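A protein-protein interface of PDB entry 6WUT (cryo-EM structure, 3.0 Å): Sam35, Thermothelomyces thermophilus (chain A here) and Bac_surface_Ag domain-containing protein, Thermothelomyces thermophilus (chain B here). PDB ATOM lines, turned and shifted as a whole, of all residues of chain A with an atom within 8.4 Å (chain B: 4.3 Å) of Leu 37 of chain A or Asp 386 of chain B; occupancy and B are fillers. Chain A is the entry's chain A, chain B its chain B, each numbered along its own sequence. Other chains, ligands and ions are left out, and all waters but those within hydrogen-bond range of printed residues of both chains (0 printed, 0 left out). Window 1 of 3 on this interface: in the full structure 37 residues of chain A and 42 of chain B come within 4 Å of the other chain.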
ATOM      1  N   PRO A  34       9.821  -1.884   1.951  1.00  0.00           N
ATOM      2  CA  PRO A  34      10.811  -1.222   2.809  1.00  0.00           C
ATOM      3  C   PRO A  34      11.110   0.204   2.373  1.00  0.00           C
ATOM      4  O   PRO A  34      10.743   0.655   1.288  1.00  0.00           O
ATOM      5  CB  PRO A  34      12.047  -2.111   2.659  1.00  0.00           C
ATOM      6  CG  PRO A  34      11.869  -2.783   1.366  1.00  0.00           C
ATOM      7  CD  PRO A  34      10.414  -3.034   1.248  1.00  0.00           C
ATOM      8  N   ASN A  35      11.770   0.929   3.264  1.00  0.00           N
ATOM      9  CA  ASN A  35      12.170   2.291   2.971  1.00  0.00           C
ATOM     10  C   ASN A  35      13.399   2.271   2.085  1.00  0.00           C
ATOM     11  O   ASN A  35      14.273   1.416   2.239  1.00  0.00           O
ATOM     12  CB  ASN A  35      12.464   3.059   4.258  1.00  0.00           C
ATOM     13  CG  ASN A  35      11.331   2.989   5.246  1.00  0.00           C
ATOM     14  OD1 ASN A  35      10.422   3.815   5.224  1.00  0.00           O
ATOM     15  ND2 ASN A  35      11.378   2.004   6.126  1.00  0.00           N
ATOM     16  N   GLU A  36      13.455   3.207   1.146  1.00  0.00           N
ATOM     17  CA  GLU A  36      14.591   3.278   0.248  1.00  0.00           C
ATOM     18  C   GLU A  36      15.816   3.804   0.980  1.00  0.00           C
ATOM     19  O   GLU A  36      15.723   4.465   2.014  1.00  0.00           O
ATOM     20  CB  GLU A  36      14.279   4.172  -0.944  1.00  0.00           C
ATOM     21  CG  GLU A  36      13.082   3.734  -1.740  1.00  0.00           C
ATOM     22  CD  GLU A  36      12.857   4.601  -2.956  1.00  0.00           C
ATOM     23  OE1 GLU A  36      13.763   5.388  -3.297  1.00  0.00           O
ATOM     24  OE2 GLU A  36      11.775   4.498  -3.571  1.00  0.00           O
ATOM     25  N   LEU A  37      16.974   3.501   0.422  1.00  0.00           N
ATOM     26  CA  LEU A  37      18.231   3.916   0.991  1.00  0.00           C
ATOM     27  C   LEU A  37      18.438   5.399   0.703  1.00  0.00           C
ATOM     28  O   LEU A  37      17.729   5.977  -0.123  1.00  0.00           O
ATOM     29  CB  LEU A  37      19.350   3.051   0.417  1.00  0.00           C
ATOM     30  CG  LEU A  37      19.289   1.563   0.744  1.00  0.00           C
ATOM     31  CD1 LEU A  37      20.262   0.816  -0.119  1.00  0.00           C
ATOM     32  CD2 LEU A  37      19.607   1.334   2.192  1.00  0.00           C
ATOM     33  N   PRO A  38      19.379   6.058   1.386  1.00  0.00           N
ATOM     34  CA  PRO A  38      19.700   7.446   1.038  1.00  0.00           C
ATOM     35  C   PRO A  38      20.305   7.577  -0.352  1.00  0.00           C
ATOM     36  O   PRO A  38      20.622   6.597  -1.026  1.00  0.00           O
ATOM     37  CB  PRO A  38      20.704   7.842   2.115  1.00  0.00           C
ATOM     38  CG  PRO A  38      20.335   7.032   3.254  1.00  0.00           C
ATOM     39  CD  PRO A  38      19.929   5.721   2.710  1.00  0.00           C
ATOM     40  N   GLU A  39      20.483   8.825  -0.778  1.00  0.00           N
ATOM     41  CA  GLU A  39      20.999   9.076  -2.117  1.00  0.00           C
ATOM     42  C   GLU A  39      22.463   8.695  -2.235  1.00  0.00           C
ATOM     43  O   GLU A  39      22.915   8.315  -3.317  1.00  0.00           O
ATOM     44  CB  GLU A  39      20.788  10.547  -2.486  1.00  0.00           C
ATOM     45  CG  GLU A  39      21.288  11.002  -3.856  1.00  0.00           C
ATOM     46  CD  GLU A  39      20.680  10.245  -5.033  1.00  0.00           C
ATOM     47  OE1 GLU A  39      19.550   9.728  -4.937  1.00  0.00           O
ATOM     48  OE2 GLU A  39      21.336  10.182  -6.088  1.00  0.00           O
ATOM     49  N   ARG A  40      23.200   8.730  -1.131  1.00  0.00           N
ATOM     50  CA  ARG A  40      24.630   8.471  -1.191  1.00  0.00           C
ATOM     51  C   ARG A  40      24.919   7.000  -1.459  1.00  0.00           C
ATOM     52  O   ARG A  40      25.784   6.673  -2.276  1.00  0.00           O
ATOM     53  CB  ARG A  40      25.280   8.938   0.104  1.00  0.00           C
ATOM     54  CG  ARG A  40      26.765   8.794   0.137  1.00  0.00           C
ATOM     55  CD  ARG A  40      27.332   9.507   1.342  1.00  0.00           C
ATOM     56  NE  ARG A  40      28.673   9.035   1.639  1.00  0.00           N
ATOM     57  CZ  ARG A  40      29.772   9.578   1.140  1.00  0.00           C
ATOM     58  NH1 ARG A  40      29.677  10.615   0.328  1.00  0.00           N
ATOM     59  NH2 ARG A  40      30.960   9.089   1.448  1.00  0.00           N
ATOM     60  N   SER A  41      24.188   6.096  -0.812  1.00  0.00           N
ATOM     61  CA  SER A  41      24.376   4.677  -1.069  1.00  0.00           C
ATOM     62  C   SER A  41      23.765   4.233  -2.385  1.00  0.00           C
ATOM     63  O   SER A  41      24.289   3.305  -3.004  1.00  0.00           O
ATOM     64  CB  SER A  41      23.789   3.848   0.062  1.00  0.00           C
ATOM     65  OG  SER A  41      22.450   4.210   0.303  1.00  0.00           O
ATOM     66  N   GLN A  42      22.707   4.896  -2.841  1.00  0.00           N
ATOM     67  CA  GLN A  42      22.136   4.631  -4.151  1.00  0.00           C
ATOM     68  C   GLN A  42      23.055   5.032  -5.291  1.00  0.00           C
ATOM     69  O   GLN A  42      22.893   4.519  -6.400  1.00  0.00           O
ATOM     70  CB  GLN A  42      20.802   5.353  -4.297  1.00  0.00           C
ATOM     71  CG  GLN A  42      19.674   4.685  -3.561  1.00  0.00           C
ATOM     72  CD  GLN A  42      18.347   5.311  -3.870  1.00  0.00           C
ATOM     73  OE1 GLN A  42      18.283   6.408  -4.413  1.00  0.00           O
ATOM     74  NE2 GLN A  42      17.272   4.618  -3.531  1.00  0.00           N
ATOM     75  N   GLN A  43      24.013   5.921  -5.048  1.00  0.00           N
ATOM     76  CA  GLN A  43      25.021   6.283  -6.033  1.00  0.00           C
ATOM     77  C   GLN A  43      26.287   5.453  -5.895  1.00  0.00           C
ATOM     78  O   GLN A  43      26.820   4.963  -6.892  1.00  0.00           O
ATOM     79  CB  GLN A  43      25.372   7.767  -5.905  1.00  0.00           C
ATOM     80  CG  GLN A  43      24.259   8.710  -6.265  1.00  0.00           C
ATOM     81  CD  GLN A  43      24.003   8.801  -7.752  1.00  0.00           C
ATOM     82  OE1 GLN A  43      24.865   8.478  -8.565  1.00  0.00           O
ATOM     83  NE2 GLN A  43      22.810   9.248  -8.117  1.00  0.00           N
ATOM     84  N   THR A  45      26.959   2.533  -3.955  1.00  0.00           N
ATOM     85  CA  THR A  45      26.908   1.090  -3.767  1.00  0.00           C
ATOM     86  C   THR A  45      25.826   0.425  -4.607  1.00  0.00           C
ATOM     87  O   THR A  45      25.107  -0.440  -4.101  1.00  0.00           O
ATOM     88  CB  THR A  45      26.695   0.739  -2.294  1.00  0.00           C
ATOM     89  OG1 THR A  45      25.300   0.538  -2.051  1.00  0.00           O
ATOM     90  CG2 THR A  45      27.183   1.845  -1.375  1.00  0.00           C
ATOM     91  N   SER A  46      25.680   0.797  -5.877  1.00  0.00           N
ATOM     92  CA  SER A  46      24.600   0.242  -6.686  1.00  0.00           C
ATOM     93  C   SER A  46      25.058  -0.225  -8.064  1.00  0.00           C
ATOM     94  O   SER A  46      24.297  -0.118  -9.030  1.00  0.00           O
ATOM     95  CB  SER A  46      23.464   1.256  -6.823  1.00  0.00           C
ATOM     96  OG  SER A  46      23.875   2.383  -7.567  1.00  0.00           O
ATOM     97  N   ARG A 108      24.856  -6.217  -5.761  1.00  0.00           N
ATOM     98  CA  ARG A 108      23.653  -6.500  -4.998  1.00  0.00           C
ATOM     99  C   ARG A 108      22.716  -7.415  -5.774  1.00  0.00           C
ATOM    100  O   ARG A 108      22.683  -7.412  -7.006  1.00  0.00           O
ATOM    101  CB  ARG A 108      22.911  -5.211  -4.668  1.00  0.00           C
ATOM    102  CG  ARG A 108      23.636  -4.247  -3.769  1.00  0.00           C
ATOM    103  CD  ARG A 108      22.743  -3.062  -3.511  1.00  0.00           C
ATOM    104  NE  ARG A 108      23.331  -2.074  -2.621  1.00  0.00           N
ATOM    105  CZ  ARG A 108      23.194  -2.081  -1.304  1.00  0.00           C
ATOM    106  NH1 ARG A 108      22.493  -3.029  -0.718  1.00  0.00           N
ATOM    107  NH2 ARG A 108      23.756  -1.135  -0.570  1.00  0.00           N
ATOM    108  N   SER A 110      19.230  -7.814  -4.251  1.00  0.00           N
ATOM    109  CA  SER A 110      18.110  -6.964  -3.903  1.00  0.00           C
ATOM    110  C   SER A 110      18.600  -5.539  -3.707  1.00  0.00           C
ATOM    111  O   SER A 110      19.785  -5.318  -3.446  1.00  0.00           O
ATOM    112  CB  SER A 110      17.440  -7.477  -2.623  1.00  0.00           C
ATOM    113  OG  SER A 110      16.775  -8.704  -2.855  1.00  0.00           O
ATOM    114  N   PRO A 111      17.726  -4.532  -3.837  1.00  0.00           N
ATOM    115  CA  PRO A 111      18.165  -3.147  -3.596  1.00  0.00           C
ATOM    116  C   PRO A 111      18.493  -2.827  -2.147  1.00  0.00           C
ATOM    117  O   PRO A 111      19.040  -1.750  -1.890  1.00  0.00           O
ATOM    118  CB  PRO A 111      16.974  -2.315  -4.082  1.00  0.00           C
ATOM    119  CG  PRO A 111      15.826  -3.242  -4.055  1.00  0.00           C
ATOM    120  CD  PRO A 111      16.385  -4.562  -4.442  1.00  0.00           C
ATOM    121  N   THR A 112      18.189  -3.713  -1.197  1.00  0.00           N
ATOM    122  CA  THR A 112      18.468  -3.488   0.215  1.00  0.00           C
ATOM    123  C   THR A 112      19.267  -4.630   0.832  1.00  0.00           C
ATOM    124  O   THR A 112      19.320  -4.747   2.058  1.00  0.00           O
ATOM    125  CB  THR A 112      17.166  -3.286   0.991  1.00  0.00           C
ATOM    126  OG1 THR A 112      16.130  -4.084   0.401  1.00  0.00           O
ATOM    127  CG2 THR A 112      16.748  -1.825   0.979  1.00  0.00           C
ATOM    128  N   ALA A 113      19.871  -5.486   0.010  1.00  0.00           N
ATOM    129  CA  ALA A 113      20.672  -6.599   0.498  1.00  0.00           C
ATOM    130  C   ALA A 113      21.815  -6.846  -0.471  1.00  0.00           C
ATOM    131  O   ALA A 113      21.618  -6.802  -1.687  1.00  0.00           O
ATOM    132  CB  ALA A 113      19.836  -7.870   0.659  1.00  0.00           C
ATOM    133  N   SER A 114      23.000  -7.108   0.068  1.00  0.00           N
ATOM    134  CA  SER A 114      24.204  -7.315  -0.718  1.00  0.00           C
ATOM    135  C   SER A 114      24.992  -8.465  -0.114  1.00  0.00           C
ATOM    136  O   SER A 114      24.935  -8.681   1.101  1.00  0.00           O
ATOM    137  CB  SER A 114      25.073  -6.048  -0.753  1.00  0.00           C
ATOM    138  OG  SER A 114      26.280  -6.243  -1.470  1.00  0.00           O
ATOM    139  N   PRO A 115      25.727  -9.234  -0.938  1.00  0.00           N
ATOM    140  CA  PRO A 115      26.515 -10.351  -0.396  1.00  0.00           C
ATOM    141  C   PRO A 115      27.703  -9.926   0.453  1.00  0.00           C
ATOM    142  O   PRO A 115      27.961  -8.733   0.641  1.00  0.00           O
ATOM    143  CB  PRO A 115      26.972 -11.098  -1.656  1.00  0.00           C
ATOM    144  CG  PRO A 115      26.793 -10.142  -2.764  1.00  0.00           C
ATOM    145  CD  PRO A 115      25.638  -9.302  -2.405  1.00  0.00           C
ATOM    146  N   SER B 255      27.315  -3.196   6.266  1.00  0.00           N
ATOM    147  CA  SER B 255      26.682  -3.079   4.964  1.00  0.00           C
ATOM    148  C   SER B 255      27.600  -2.333   4.012  1.00  0.00           C
ATOM    149  O   SER B 255      28.609  -1.773   4.429  1.00  0.00           O
ATOM    150  CB  SER B 255      25.346  -2.366   5.120  1.00  0.00           C
ATOM    151  OG  SER B 255      25.532  -1.067   5.638  1.00  0.00           O
ATOM    152  N   PRO B 256      27.305  -2.344   2.707  1.00  0.00           N
ATOM    153  CA  PRO B 256      28.032  -1.447   1.796  1.00  0.00           C
ATOM    154  C   PRO B 256      27.820   0.037   2.063  1.00  0.00           C
ATOM    155  O   PRO B 256      28.686   0.846   1.710  1.00  0.00           O
ATOM    156  CB  PRO B 256      27.482  -1.851   0.428  1.00  0.00           C
ATOM    157  CG  PRO B 256      27.145  -3.265   0.581  1.00  0.00           C
ATOM    158  CD  PRO B 256      26.652  -3.439   1.964  1.00  0.00           C
ATOM    159  N   THR B 257      26.694   0.417   2.673  1.00  0.00           N
ATOM    160  CA  THR B 257      26.441   1.815   3.013  1.00  0.00           C
ATOM    161  C   THR B 257      27.362   2.289   4.126  1.00  0.00           C
ATOM    162  O   THR B 257      27.806   3.441   4.125  1.00  0.00           O
ATOM    163  CB  THR B 257      24.981   1.984   3.430  1.00  0.00           C
ATOM    164  OG1 THR B 257      24.129   1.402   2.440  1.00  0.00           O
ATOM    165  CG2 THR B 257      24.616   3.442   3.598  1.00  0.00           C
ATOM    166  N   PRO B 384      15.563   3.399   7.001  1.00  0.00           N
ATOM    167  CA  PRO B 384      16.168   2.584   5.945  1.00  0.00           C
ATOM    168  C   PRO B 384      17.171   1.616   6.548  1.00  0.00           C
ATOM    169  O   PRO B 384      18.013   2.001   7.357  1.00  0.00           O
ATOM    170  CB  PRO B 384      16.855   3.620   5.048  1.00  0.00           C
ATOM    171  CG  PRO B 384      16.229   4.926   5.414  1.00  0.00           C
ATOM    172  CD  PRO B 384      15.902   4.821   6.853  1.00  0.00           C
ATOM    173  N   HIS B 385      17.066   0.350   6.171  1.00  0.00           N
ATOM    174  CA  HIS B 385      17.996  -0.668   6.629  1.00  0.00           C
ATOM    175  C   HIS B 385      18.698  -1.272   5.429  1.00  0.00           C
ATOM    176  O   HIS B 385      18.041  -1.722   4.488  1.00  0.00           O
ATOM    177  CB  HIS B 385      17.287  -1.763   7.428  1.00  0.00           C
ATOM    178  CG  HIS B 385      16.996  -1.394   8.850  1.00  0.00           C
ATOM    179  ND1 HIS B 385      17.738  -1.870   9.905  1.00  0.00           N
ATOM    180  CD2 HIS B 385      16.029  -0.620   9.391  1.00  0.00           C
ATOM    181  CE1 HIS B 385      17.248  -1.399  11.035  1.00  0.00           C
ATOM    182  NE2 HIS B 385      16.213  -0.635  10.750  1.00  0.00           N
ATOM    183  N   ASP B 386      20.026  -1.284   5.459  1.00  0.00           N
ATOM    184  CA  ASP B 386      20.834  -1.947   4.441  1.00  0.00           C
ATOM    185  C   ASP B 386      21.264  -3.286   5.022  1.00  0.00           C
ATOM    186  O   ASP B 386      22.273  -3.376   5.720  1.00  0.00           O
ATOM    187  CB  ASP B 386      22.031  -1.094   4.045  1.00  0.00           C
ATOM    188  CG  ASP B 386      22.589  -1.467   2.692  1.00  0.00           C
ATOM    189  OD1 ASP B 386      22.162  -2.492   2.132  1.00  0.00           O
ATOM    190  OD2 ASP B 386      23.449  -0.730   2.178  1.00  0.00           O
ATOM    191  N   GLY B 387      20.501  -4.328   4.730  1.00  0.00           N
ATOM    192  CA  GLY B 387      20.749  -5.591   5.389  1.00  0.00           C
ATOM    193  C   GLY B 387      20.213  -5.520   6.800  1.00  0.00           C
ATOM    194  O   GLY B 387      19.001  -5.434   7.024  1.00  0.00           O
ATOM    195  N   VAL B 388      21.118  -5.563   7.772  1.00  0.00           N
ATOM    196  CA  VAL B 388      20.732  -5.433   9.169  1.00  0.00           C
ATOM    197  C   VAL B 388      21.103  -4.079   9.753  1.00  0.00           C
ATOM    198  O   VAL B 388      20.605  -3.731  10.834  1.00  0.00           O
ATOM    199  CB  VAL B 388      21.349  -6.553  10.030  1.00  0.00           C
ATOM    200  CG1 VAL B 388      20.801  -7.900   9.621  1.00  0.00           C
ATOM    201  CG2 VAL B 388      22.858  -6.530   9.930  1.00  0.00           C
ATOM    202  N   ASP B 389      21.962  -3.313   9.087  1.00  0.00           N
ATOM    203  CA  ASP B 389      22.426  -2.056   9.650  1.00  0.00           C
ATOM    204  C   ASP B 389      21.348  -0.995   9.543  1.00  0.00           C
ATOM    205  O   ASP B 389      20.597  -0.948   8.573  1.00  0.00           O
ATOM    206  CB  ASP B 389      23.690  -1.587   8.941  1.00  0.00           C
ATOM    207  CG  ASP B 389      24.884  -2.436   9.273  1.00  0.00           C
ATOM    208  OD1 ASP B 389      24.698  -3.524   9.851  1.00  0.00           O
ATOM    209  OD2 ASP B 389      26.012  -2.013   8.969  1.00  0.00           O
ATOM    210  N   ALA B 429      14.284   8.675   3.934  1.00  0.00           N
ATOM    211  CA  ALA B 429      15.538   9.209   3.444  1.00  0.00           C
ATOM    212  C   ALA B 429      15.268  10.178   2.301  1.00  0.00           C
ATOM    213  O   ALA B 429      14.124  10.516   1.993  1.00  0.00           O
ATOM    214  CB  ALA B 429      16.458   8.067   3.026  1.00  0.00           C
ATOM    215  N   ASN B 431      16.404  11.025  -1.732  1.00  0.00           N
ATOM    216  CA  ASN B 431      17.069  10.582  -2.943  1.00  0.00           C
ATOM    217  C   ASN B 431      16.768  11.557  -4.073  1.00  0.00           C
ATOM    218  O   ASN B 431      16.039  12.535  -3.903  1.00  0.00           O
ATOM    219  CB  ASN B 431      16.657   9.153  -3.321  1.00  0.00           C
ATOM    220  CG  ASN B 431      15.211   8.866  -3.026  1.00  0.00           C
ATOM    221  OD1 ASN B 431      14.335   9.677  -3.313  1.00  0.00           O
ATOM    222  ND2 ASN B 431      14.947   7.710  -2.440  1.00  0.00           N
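OE1 of Glu 36 of chain A is in hydrogen-bond range of ND2 of Asn 431 of chain B, at 2.7 Å. The side-chain carboxylate (OD2) of Asp 386 of chain B lies within salt-bridge range of the guanidinium group (NH2) of Arg 108 of chain A, at 2.8 Å. O of Thr 112 of chain A lies within hydrogen-bond range of N of Gly 387 of chain B (3.0 Å).
The backbone carbonyl oxygen of Pro 38 of chain A lies within hydrogen-bond range of the side-chain hydroxyl of Ser 41 of chain A. The side-chain amide nitrogen of Gln 43 of chain A lies within hydrogen-bond range of the side-chain carboxylate of Glu 39 of chain A, at 2.7 Å. The backbone carbonyl oxygen of Ser 41 of chain A sits at hydrogen-bond distance from the side-chain hydroxyl of Thr 45 of chain A. NH2 of Arg 108 of chain A is in hydrogen-bond range of OG1 of Thr 45 of chain A, at 2.7 Å. OD2 of Asp 386 of chain B sits close to N of Thr 257 of chain B (3.5 Å). O of Asp 389 of chain B sits close to ND1 of His 385 of chain B (3.3 Å).
Glu 36 of chain A touches Pro 384 of chain B (O to CB, 3.3 Å). Ala 429 of chain B touches Glu 36 of chain A. Asn 431 of chain B touches Glu 39 of chain A (CA to OE1, 3.3 Å). Thr 257 of chain B touches Ser 41 of chain A. Gln 42 of chain A touches Asn 431 of chain B. Thr 45 of chain A touches Pro 256 of chain B (CG2 to O, 3.6 Å). Arg 108 of chain A touches Pro 256 of chain B (NH2 to CB, 3.9 Å). Thr 257 of chain B touches Arg 108 of chain A. His 385 of chain B touches Thr 112 of chain A (O to CG2, 3.7 Å). Ser 114 of chain A touches Pro 256 of chain B.
Of the printed residues of chain B, Leu 37 of chain A touches Asp 386 (3.9 Å) and Ala 429 (3.99 Å). Asp 386 of chain B touches just these residues of chain A: Leu 37, Arg 108 and Thr 112. Of chain A, only Thr 112 (3.0 Å) comes within 4 Å of Gly 387 of chain B. Printed residues of chain B within 4 Å of Thr 112 of chain A: His 385 (3.7 Å), Asp 386 (3.6 Å) and Gly 387 (3.0 Å). Of the printed residues of chain B, Ser 41 of chain A touches Thr 257 (3.4 Å). Of the printed residues of chain A, Pro 256 of chain B touches Thr 45, Arg 108 and Ser 114. Of the printed residues of chain A, His 385 of chain B touches Thr 112 (3.7 Å). Gln 43 of chain A touches none of the printed residues of chain B. Ser 255 of chain B touches none of the printed residues of chain A. The nearest printed residue of chain B that does not touch Leu 37 of chain A is Asn 431 of chain B (4.01 Å). The nearest residue of chain A that does not touch Asp 386 of chain B is Ala 113 of chain A (4.3 Å).
Of the 11 printed residues of chain B, 8 touch a printed residue of chain A. Of the 19 printed residues of chain A, 10 touch a printed residue of chain B. Printed residues of chain A that touch a printed residue of chain B: Glu 36, Leu 37, Pro 38, Glu 39, Ser 41, Gln 42, Thr 45, Arg 108, Thr 112 and Ser 114. Among the printed residues, 17 pairs touch across the chains. Among the printed residues, Asp or Glu carboxylates within 4 Å of a Lys or Arg side-chain nitrogen of the other chain: Arg 108 of chain A with Asp 386 of chain B (2.8 Å).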
